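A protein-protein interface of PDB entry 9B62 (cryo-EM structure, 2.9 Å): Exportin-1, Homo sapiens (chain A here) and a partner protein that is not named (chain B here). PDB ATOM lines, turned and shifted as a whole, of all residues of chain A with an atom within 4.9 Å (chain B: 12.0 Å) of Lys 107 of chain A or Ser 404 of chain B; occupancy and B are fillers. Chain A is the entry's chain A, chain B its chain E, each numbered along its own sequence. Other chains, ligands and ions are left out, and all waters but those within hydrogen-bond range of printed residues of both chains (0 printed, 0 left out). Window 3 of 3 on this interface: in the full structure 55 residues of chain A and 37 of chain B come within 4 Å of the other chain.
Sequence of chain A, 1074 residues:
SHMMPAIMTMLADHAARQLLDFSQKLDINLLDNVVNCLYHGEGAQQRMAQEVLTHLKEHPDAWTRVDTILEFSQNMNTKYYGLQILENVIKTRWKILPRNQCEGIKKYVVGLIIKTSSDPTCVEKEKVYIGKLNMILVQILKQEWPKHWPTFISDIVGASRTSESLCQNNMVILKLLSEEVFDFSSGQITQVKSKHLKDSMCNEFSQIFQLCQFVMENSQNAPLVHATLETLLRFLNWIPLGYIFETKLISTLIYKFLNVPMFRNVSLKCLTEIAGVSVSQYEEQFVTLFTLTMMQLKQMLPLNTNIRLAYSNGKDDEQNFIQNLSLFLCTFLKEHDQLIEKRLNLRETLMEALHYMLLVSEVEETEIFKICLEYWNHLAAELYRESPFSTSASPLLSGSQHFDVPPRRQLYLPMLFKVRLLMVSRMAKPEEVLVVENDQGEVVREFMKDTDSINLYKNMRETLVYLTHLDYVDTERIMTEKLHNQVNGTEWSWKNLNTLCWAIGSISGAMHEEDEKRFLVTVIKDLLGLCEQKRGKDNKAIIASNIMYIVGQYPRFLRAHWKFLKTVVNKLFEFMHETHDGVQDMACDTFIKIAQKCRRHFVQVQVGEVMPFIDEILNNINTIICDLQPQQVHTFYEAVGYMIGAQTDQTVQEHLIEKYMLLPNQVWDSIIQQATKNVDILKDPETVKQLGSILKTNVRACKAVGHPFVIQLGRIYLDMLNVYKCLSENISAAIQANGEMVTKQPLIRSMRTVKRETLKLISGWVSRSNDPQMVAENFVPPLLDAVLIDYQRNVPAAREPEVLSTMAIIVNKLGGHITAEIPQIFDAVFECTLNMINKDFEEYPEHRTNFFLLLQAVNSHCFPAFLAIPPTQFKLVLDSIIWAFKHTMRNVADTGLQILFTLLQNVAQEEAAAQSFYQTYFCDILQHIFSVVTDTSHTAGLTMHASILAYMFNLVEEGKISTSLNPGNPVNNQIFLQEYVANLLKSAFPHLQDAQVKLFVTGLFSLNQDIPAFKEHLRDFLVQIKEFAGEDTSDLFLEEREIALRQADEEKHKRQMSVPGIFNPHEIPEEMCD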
ATOM      1  N   GLU A 103       8.542   5.942  29.783  1.00  0.00           N
ATOM      2  CA  GLU A 103       8.333   4.499  29.767  1.00  0.00           C
ATOM      3  C   GLU A 103       7.697   4.055  28.458  1.00  0.00           C
ATOM      4  O   GLU A 103       8.069   3.017  27.900  1.00  0.00           O
ATOM      5  CB  GLU A 103       7.464   4.083  30.954  1.00  0.00           C
ATOM      6  CG  GLU A 103       8.089   4.352  32.312  1.00  0.00           C
ATOM      7  CD  GLU A 103       9.305   3.489  32.579  1.00  0.00           C
ATOM      8  OE1 GLU A 103       9.563   2.559  31.785  1.00  0.00           O
ATOM      9  OE2 GLU A 103      10.004   3.739  33.582  1.00  0.00           O
ATOM     10  N   GLY A 104       6.731   4.825  27.955  1.00  0.00           N
ATOM     11  CA  GLY A 104       6.108   4.472  26.691  1.00  0.00           C
ATOM     12  C   GLY A 104       7.096   4.461  25.542  1.00  0.00           C
ATOM     13  O   GLY A 104       7.112   3.534  24.731  1.00  0.00           O
ATOM     14  N   ILE A 105       7.939   5.492  25.460  1.00  0.00           N
ATOM     15  CA  ILE A 105       8.934   5.552  24.391  1.00  0.00           C
ATOM     16  C   ILE A 105       9.906   4.386  24.510  1.00  0.00           C
ATOM     17  O   ILE A 105      10.248   3.734  23.517  1.00  0.00           O
ATOM     18  CB  ILE A 105       9.677   6.899  24.417  1.00  0.00           C
ATOM     19  CG1 ILE A 105       8.714   8.050  24.132  1.00  0.00           C
ATOM     20  CG2 ILE A 105      10.809   6.892  23.403  1.00  0.00           C
ATOM     21  CD1 ILE A 105       9.324   9.414  24.335  1.00  0.00           C
ATOM     22  N   LYS A 106      10.378   4.116  25.729  1.00  0.00           N
ATOM     23  CA  LYS A 106      11.317   3.018  25.934  1.00  0.00           C
ATOM     24  C   LYS A 106      10.709   1.694  25.487  1.00  0.00           C
ATOM     25  O   LYS A 106      11.336   0.923  24.748  1.00  0.00           O
ATOM     26  CB  LYS A 106      11.714   2.957  27.409  1.00  0.00           C
ATOM     27  CG  LYS A 106      12.759   1.915  27.752  1.00  0.00           C
ATOM     28  CD  LYS A 106      12.726   1.567  29.233  1.00  0.00           C
ATOM     29  CE  LYS A 106      12.895   2.797  30.111  1.00  0.00           C
ATOM     30  NZ  LYS A 106      12.938   2.442  31.554  1.00  0.00           N
ATOM     31  N   LYS A 107       9.482   1.416  25.929  1.00  0.00           N
ATOM     32  CA  LYS A 107       8.840   0.154  25.586  1.00  0.00           C
ATOM     33  C   LYS A 107       8.592   0.054  24.088  1.00  0.00           C
ATOM     34  O   LYS A 107       8.786  -1.009  23.491  1.00  0.00           O
ATOM     35  CB  LYS A 107       7.531   0.010  26.359  1.00  0.00           C
ATOM     36  CG  LYS A 107       6.911  -1.367  26.264  1.00  0.00           C
ATOM     37  CD  LYS A 107       5.639  -1.463  27.086  1.00  0.00           C
ATOM     38  CE  LYS A 107       5.091  -2.880  27.092  1.00  0.00           C
ATOM     39  NZ  LYS A 107       4.787  -3.374  25.722  1.00  0.00           N
ATOM     40  N   TYR A 108       8.160   1.151  23.462  1.00  0.00           N
ATOM     41  CA  TYR A 108       7.916   1.142  22.025  1.00  0.00           C
ATOM     42  C   TYR A 108       9.194   0.842  21.255  1.00  0.00           C
ATOM     43  O   TYR A 108       9.201   0.016  20.334  1.00  0.00           O
ATOM     44  CB  TYR A 108       7.330   2.489  21.602  1.00  0.00           C
ATOM     45  CG  TYR A 108       6.984   2.593  20.137  1.00  0.00           C
ATOM     46  CD1 TYR A 108       5.788   2.094  19.651  1.00  0.00           C
ATOM     47  CD2 TYR A 108       7.848   3.207  19.243  1.00  0.00           C
ATOM     48  CE1 TYR A 108       5.464   2.192  18.316  1.00  0.00           C
ATOM     49  CE2 TYR A 108       7.534   3.310  17.906  1.00  0.00           C
ATOM     50  CZ  TYR A 108       6.340   2.801  17.448  1.00  0.00           C
ATOM     51  OH  TYR A 108       6.019   2.899  16.116  1.00  0.00           O
ATOM     52  N   VAL A 109      10.295   1.503  21.623  1.00  0.00           N
ATOM     53  CA  VAL A 109      11.553   1.296  20.909  1.00  0.00           C
ATOM     54  C   VAL A 109      12.045  -0.132  21.093  1.00  0.00           C
ATOM     55  O   VAL A 109      12.499  -0.773  20.139  1.00  0.00           O
ATOM     56  CB  VAL A 109      12.603   2.320  21.374  1.00  0.00           C
ATOM     57  CG1 VAL A 109      13.962   1.975  20.801  1.00  0.00           C
ATOM     58  CG2 VAL A 109      12.191   3.720  20.957  1.00  0.00           C
ATOM     59  N   VAL A 110      11.973  -0.653  22.321  1.00  0.00           N
ATOM     60  CA  VAL A 110      12.447  -2.014  22.556  1.00  0.00           C
ATOM     61  C   VAL A 110      11.588  -3.020  21.801  1.00  0.00           C
ATOM     62  O   VAL A 110      12.102  -3.993  21.235  1.00  0.00           O
ATOM     63  CB  VAL A 110      12.485  -2.314  24.064  1.00  0.00           C
ATOM     64  CG1 VAL A 110      12.810  -3.775  24.304  1.00  0.00           C
ATOM     65  CG2 VAL A 110      13.504  -1.425  24.749  1.00  0.00           C
ATOM     66  N   GLY A 111      10.270  -2.812  21.783  1.00  0.00           N
ATOM     67  CA  GLY A 111       9.405  -3.701  21.030  1.00  0.00           C
ATOM     68  C   GLY A 111       9.699  -3.673  19.543  1.00  0.00           C
ATOM     69  O   GLY A 111       9.722  -4.716  18.888  1.00  0.00           O
ATOM     70  N   LEU A 112       9.928  -2.481  18.989  1.00  0.00           N
ATOM     71  CA  LEU A 112      10.297  -2.389  17.580  1.00  0.00           C
ATOM     72  C   LEU A 112      11.603  -3.120  17.307  1.00  0.00           C
ATOM     73  O   LEU A 112      11.726  -3.833  16.304  1.00  0.00           O
ATOM     74  CB  LEU A 112      10.421  -0.927  17.155  1.00  0.00           C
ATOM     75  CG  LEU A 112       9.161  -0.203  16.689  1.00  0.00           C
ATOM     76  CD1 LEU A 112       9.509   1.221  16.305  1.00  0.00           C
ATOM     77  CD2 LEU A 112       8.511  -0.925  15.524  1.00  0.00           C
ATOM     78  N   GLY B 400       1.174   9.203  26.787  1.00  0.00           N
ATOM     79  CA  GLY B 400       1.791   8.005  26.251  1.00  0.00           C
ATOM     80  C   GLY B 400       2.404   8.230  24.885  1.00  0.00           C
ATOM     81  O   GLY B 400       2.381   9.344  24.361  1.00  0.00           O
ATOM     82  N   PHE B 401       2.956   7.164  24.302  1.00  0.00           N
ATOM     83  CA  PHE B 401       3.580   7.244  22.979  1.00  0.00           C
ATOM     84  C   PHE B 401       3.372   5.895  22.290  1.00  0.00           C
ATOM     85  O   PHE B 401       4.157   4.963  22.474  1.00  0.00           O
ATOM     86  CB  PHE B 401       5.056   7.599  23.086  1.00  0.00           C
ATOM     87  CG  PHE B 401       5.765   7.648  21.764  1.00  0.00           C
ATOM     88  CD1 PHE B 401       6.372   6.519  21.245  1.00  0.00           C
ATOM     89  CD2 PHE B 401       5.836   8.827  21.046  1.00  0.00           C
ATOM     90  CE1 PHE B 401       7.028   6.565  20.035  1.00  0.00           C
ATOM     91  CE2 PHE B 401       6.490   8.876  19.836  1.00  0.00           C
ATOM     92  CZ  PHE B 401       7.089   7.744  19.331  1.00  0.00           C
ATOM     93  N   GLY B 402       2.310   5.809  21.493  1.00  0.00           N
ATOM     94  CA  GLY B 402       2.033   4.606  20.734  1.00  0.00           C
ATOM     95  C   GLY B 402       2.016   3.351  21.581  1.00  0.00           C
ATOM     96  O   GLY B 402       2.908   2.506  21.454  1.00  0.00           O
ATOM     97  N   SER B 403       1.021   3.224  22.456  1.00  0.00           N
ATOM     98  CA  SER B 403       0.899   2.042  23.301  1.00  0.00           C
ATOM     99  C   SER B 403       1.042   0.778  22.466  1.00  0.00           C
ATOM    100  O   SER B 403       0.227   0.511  21.579  1.00  0.00           O
ATOM    101  CB  SER B 403      -0.448   2.052  24.023  1.00  0.00           C
ATOM    102  OG  SER B 403      -0.599   0.898  24.830  1.00  0.00           O
ATOM    103  N   SER B 404       2.080   0.000  22.759  1.00  0.00           N
ATOM    104  CA  SER B 404       2.456  -1.152  21.955  1.00  0.00           C
ATOM    105  C   SER B 404       2.261  -2.443  22.738  1.00  0.00           C
ATOM    106  O   SER B 404       2.420  -2.481  23.962  1.00  0.00           O
ATOM    107  CB  SER B 404       3.915  -1.048  21.502  1.00  0.00           C
ATOM    108  OG  SER B 404       4.792  -1.080  22.615  1.00  0.00           O
ATOM    109  N   THR B 405       1.914  -3.502  22.012  1.00  0.00           N
ATOM    110  CA  THR B 405       1.798  -4.841  22.569  1.00  0.00           C
ATOM    111  C   THR B 405       3.044  -5.679  22.312  1.00  0.00           C
ATOM    112  O   THR B 405       2.998  -6.904  22.458  1.00  0.00           O
ATOM    113  CB  THR B 405       0.571  -5.550  21.991  1.00  0.00           C
ATOM    114  OG1 THR B 405       0.734  -5.725  20.578  1.00  0.00           O
ATOM    115  CG2 THR B 405      -0.691  -4.739  22.256  1.00  0.00           C
ATOM    116  N   GLY B 406       4.151  -5.047  21.935  1.00  0.00           N
ATOM    117  CA  GLY B 406       5.352  -5.777  21.598  1.00  0.00           C
ATOM    118  C   GLY B 406       6.006  -6.413  22.808  1.00  0.00           C
ATOM    119  O   GLY B 406       5.629  -6.196  23.960  1.00  0.00           O
ATOM    120  N   LEU B 407       7.017  -7.228  22.524  1.00  0.00           N
ATOM    121  CA  LEU B 407       7.715  -7.984  23.553  1.00  0.00           C
ATOM    122  C   LEU B 407       8.781  -7.096  24.194  1.00  0.00           C
ATOM    123  O   LEU B 407       8.878  -5.898  23.915  1.00  0.00           O
ATOM    124  CB  LEU B 407       8.302  -9.257  22.947  1.00  0.00           C
ATOM    125  CG  LEU B 407       8.340 -10.507  23.826  1.00  0.00           C
ATOM    126  CD1 LEU B 407       6.948 -10.894  24.299  1.00  0.00           C
ATOM    127  CD2 LEU B 407       8.977 -11.650  23.064  1.00  0.00           C
ATOM    128  N   SER B 408       9.595  -7.676  25.073  1.00  0.00           N
ATOM    129  CA  SER B 408      10.648  -6.934  25.747  1.00  0.00           C
ATOM    130  C   SER B 408      11.794  -7.880  26.070  1.00  0.00           C
ATOM    131  O   SER B 408      11.626  -9.102  26.101  1.00  0.00           O
ATOM    132  CB  SER B 408      10.131  -6.264  27.024  1.00  0.00           C
ATOM    133  OG  SER B 408       9.550  -7.216  27.896  1.00  0.00           O
ATOM    134  N   PHE B 409      12.970  -7.298  26.310  1.00  0.00           N
ATOM    135  CA  PHE B 409      14.137  -8.108  26.641  1.00  0.00           C
ATOM    136  C   PHE B 409      13.914  -8.891  27.927  1.00  0.00           C
ATOM    137  O   PHE B 409      14.285 -10.066  28.019  1.00  0.00           O
ATOM    138  CB  PHE B 409      15.378  -7.223  26.768  1.00  0.00           C
ATOM    139  CG  PHE B 409      15.848  -6.637  25.465  1.00  0.00           C
ATOM    140  CD1 PHE B 409      15.871  -7.398  24.312  1.00  0.00           C
ATOM    141  CD2 PHE B 409      16.271  -5.323  25.399  1.00  0.00           C
ATOM    142  CE1 PHE B 409      16.304  -6.859  23.120  1.00  0.00           C
ATOM    143  CE2 PHE B 409      16.703  -4.780  24.209  1.00  0.00           C
ATOM    144  CZ  PHE B 409      16.720  -5.549  23.068  1.00  0.00           C
ATOM    145  N   ALA B 410      13.308  -8.258  28.933  1.00  0.00           N
ATOM    146  CA  ALA B 410      13.065  -8.949  30.193  1.00  0.00           C
ATOM    147  C   ALA B 410      12.158 -10.154  29.993  1.00  0.00           C
ATOM    148  O   ALA B 410      12.401 -11.225  30.562  1.00  0.00           O
ATOM    149  CB  ALA B 410      12.457  -7.984  31.210  1.00  0.00           C
ATOM    150  N   ASP B 411      11.101  -9.999  29.192  1.00  0.00           N
ATOM    151  CA  ASP B 411      10.204 -11.120  28.939  1.00  0.00           C
ATOM    152  C   ASP B 411      10.918 -12.238  28.189  1.00  0.00           C
ATOM    153  O   ASP B 411      10.748 -13.419  28.513  1.00  0.00           O
ATOM    154  CB  ASP B 411       8.981 -10.642  28.157  1.00  0.00           C
ATOM    155  CG  ASP B 411       7.870 -11.672  28.124  1.00  0.00           C
ATOM    156  OD1 ASP B 411       8.172 -12.877  27.992  1.00  0.00           O
ATOM    157  OD2 ASP B 411       6.690 -11.277  28.233  1.00  0.00           O
ATOM    158  N   LEU B 412      11.720 -11.888  27.181  1.00  0.00           N
ATOM    159  CA  LEU B 412      12.456 -12.908  26.441  1.00  0.00           C
ATOM    160  C   LEU B 412      13.448 -13.634  27.339  1.00  0.00           C
ATOM    161  O   LEU B 412      13.570 -14.863  27.276  1.00  0.00           O
ATOM    162  CB  LEU B 412      13.183 -12.276  25.254  1.00  0.00           C
ATOM    163  CG  LEU B 412      12.329 -11.943  24.032  1.00  0.00           C
ATOM    164  CD1 LEU B 412      13.134 -11.133  23.040  1.00  0.00           C
ATOM    165  CD2 LEU B 412      11.810 -13.212  23.384  1.00  0.00           C
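The side-chain amino group of Lys 107 of chain A lies within hydrogen-bond range of the backbone carbonyl oxygen of Ser 404 of chain B (3.1 Å). The side-chain amino group (NZ) of Lys 107 of chain A sits at hydrogen-bond distance from the backbone carbonyl oxygen (O) of Gly 406 of chain B (3.4 Å).
Among the printed residues, merely in contact across the chains: Tyr 108 of chain A with Gly 402 of chain B (3.4 Å), Tyr 108 of chain A with Phe 401 of chain B (3.5 Å), Gly 111 of chain A with Leu 407 of chain B (3.7 Å), Ile 105 of chain A with Phe 401 of chain B (3.8 Å), Tyr 108 of chain A with Ser 404 of chain B (3.9 Å), Val 110 of chain A with Phe 409 of chain B (3.9 Å) and Gly 104 of chain A with Phe 401 of chain B (3.98 Å).
Of chain B, only Ser 404 and Gly 406 come within 4 Å of Lys 107 of chain A. Of chain A, only Lys 107 and Tyr 108 come within 4 Å of Ser 404 of chain B. No residue of chain B comes within 4 Å of Lys 106 of chain A. No residue of chain B comes within 4 Å of Val 109 of chain A. Of chain B, only Phe 409 (3.9 Å) comes within 4 Å of Val 110 of chain A. Of chain B, only Leu 407 comes within 4 Å of Gly 111 of chain A. Printed residues of chain A within 4 Å of Phe 401 of chain B: Gly 104, Ile 105 and Tyr 108. Of the printed residues of chain A, Gly 402 of chain B touches Tyr 108. The nearest residue of chain B that does not touch Lys 107 of chain A is Thr 405 of chain B (4.5 Å). The nearest printed residue of chain A that does not touch Ser 404 of chain B is Gly 111 of chain A (5.5 Å). The nearest printed residue of chain A that does not touch Leu 407 of chain B is Val 110 of chain A (4.5 Å).
Printed residues of chain B that touch a printed residue of chain A: Phe 401, Gly 402, Ser 404, Gly 406, Leu 407 and Phe 409. Printed residues of chain A that touch a printed residue of chain B: Gly 104, Ile 105, Lys 107, Tyr 108, Val 110 and Gly 111. Hydrophobic or aromatic side chains of chain A that line the printed part of chain B: Ile 105, Tyr 108 and Val 110.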
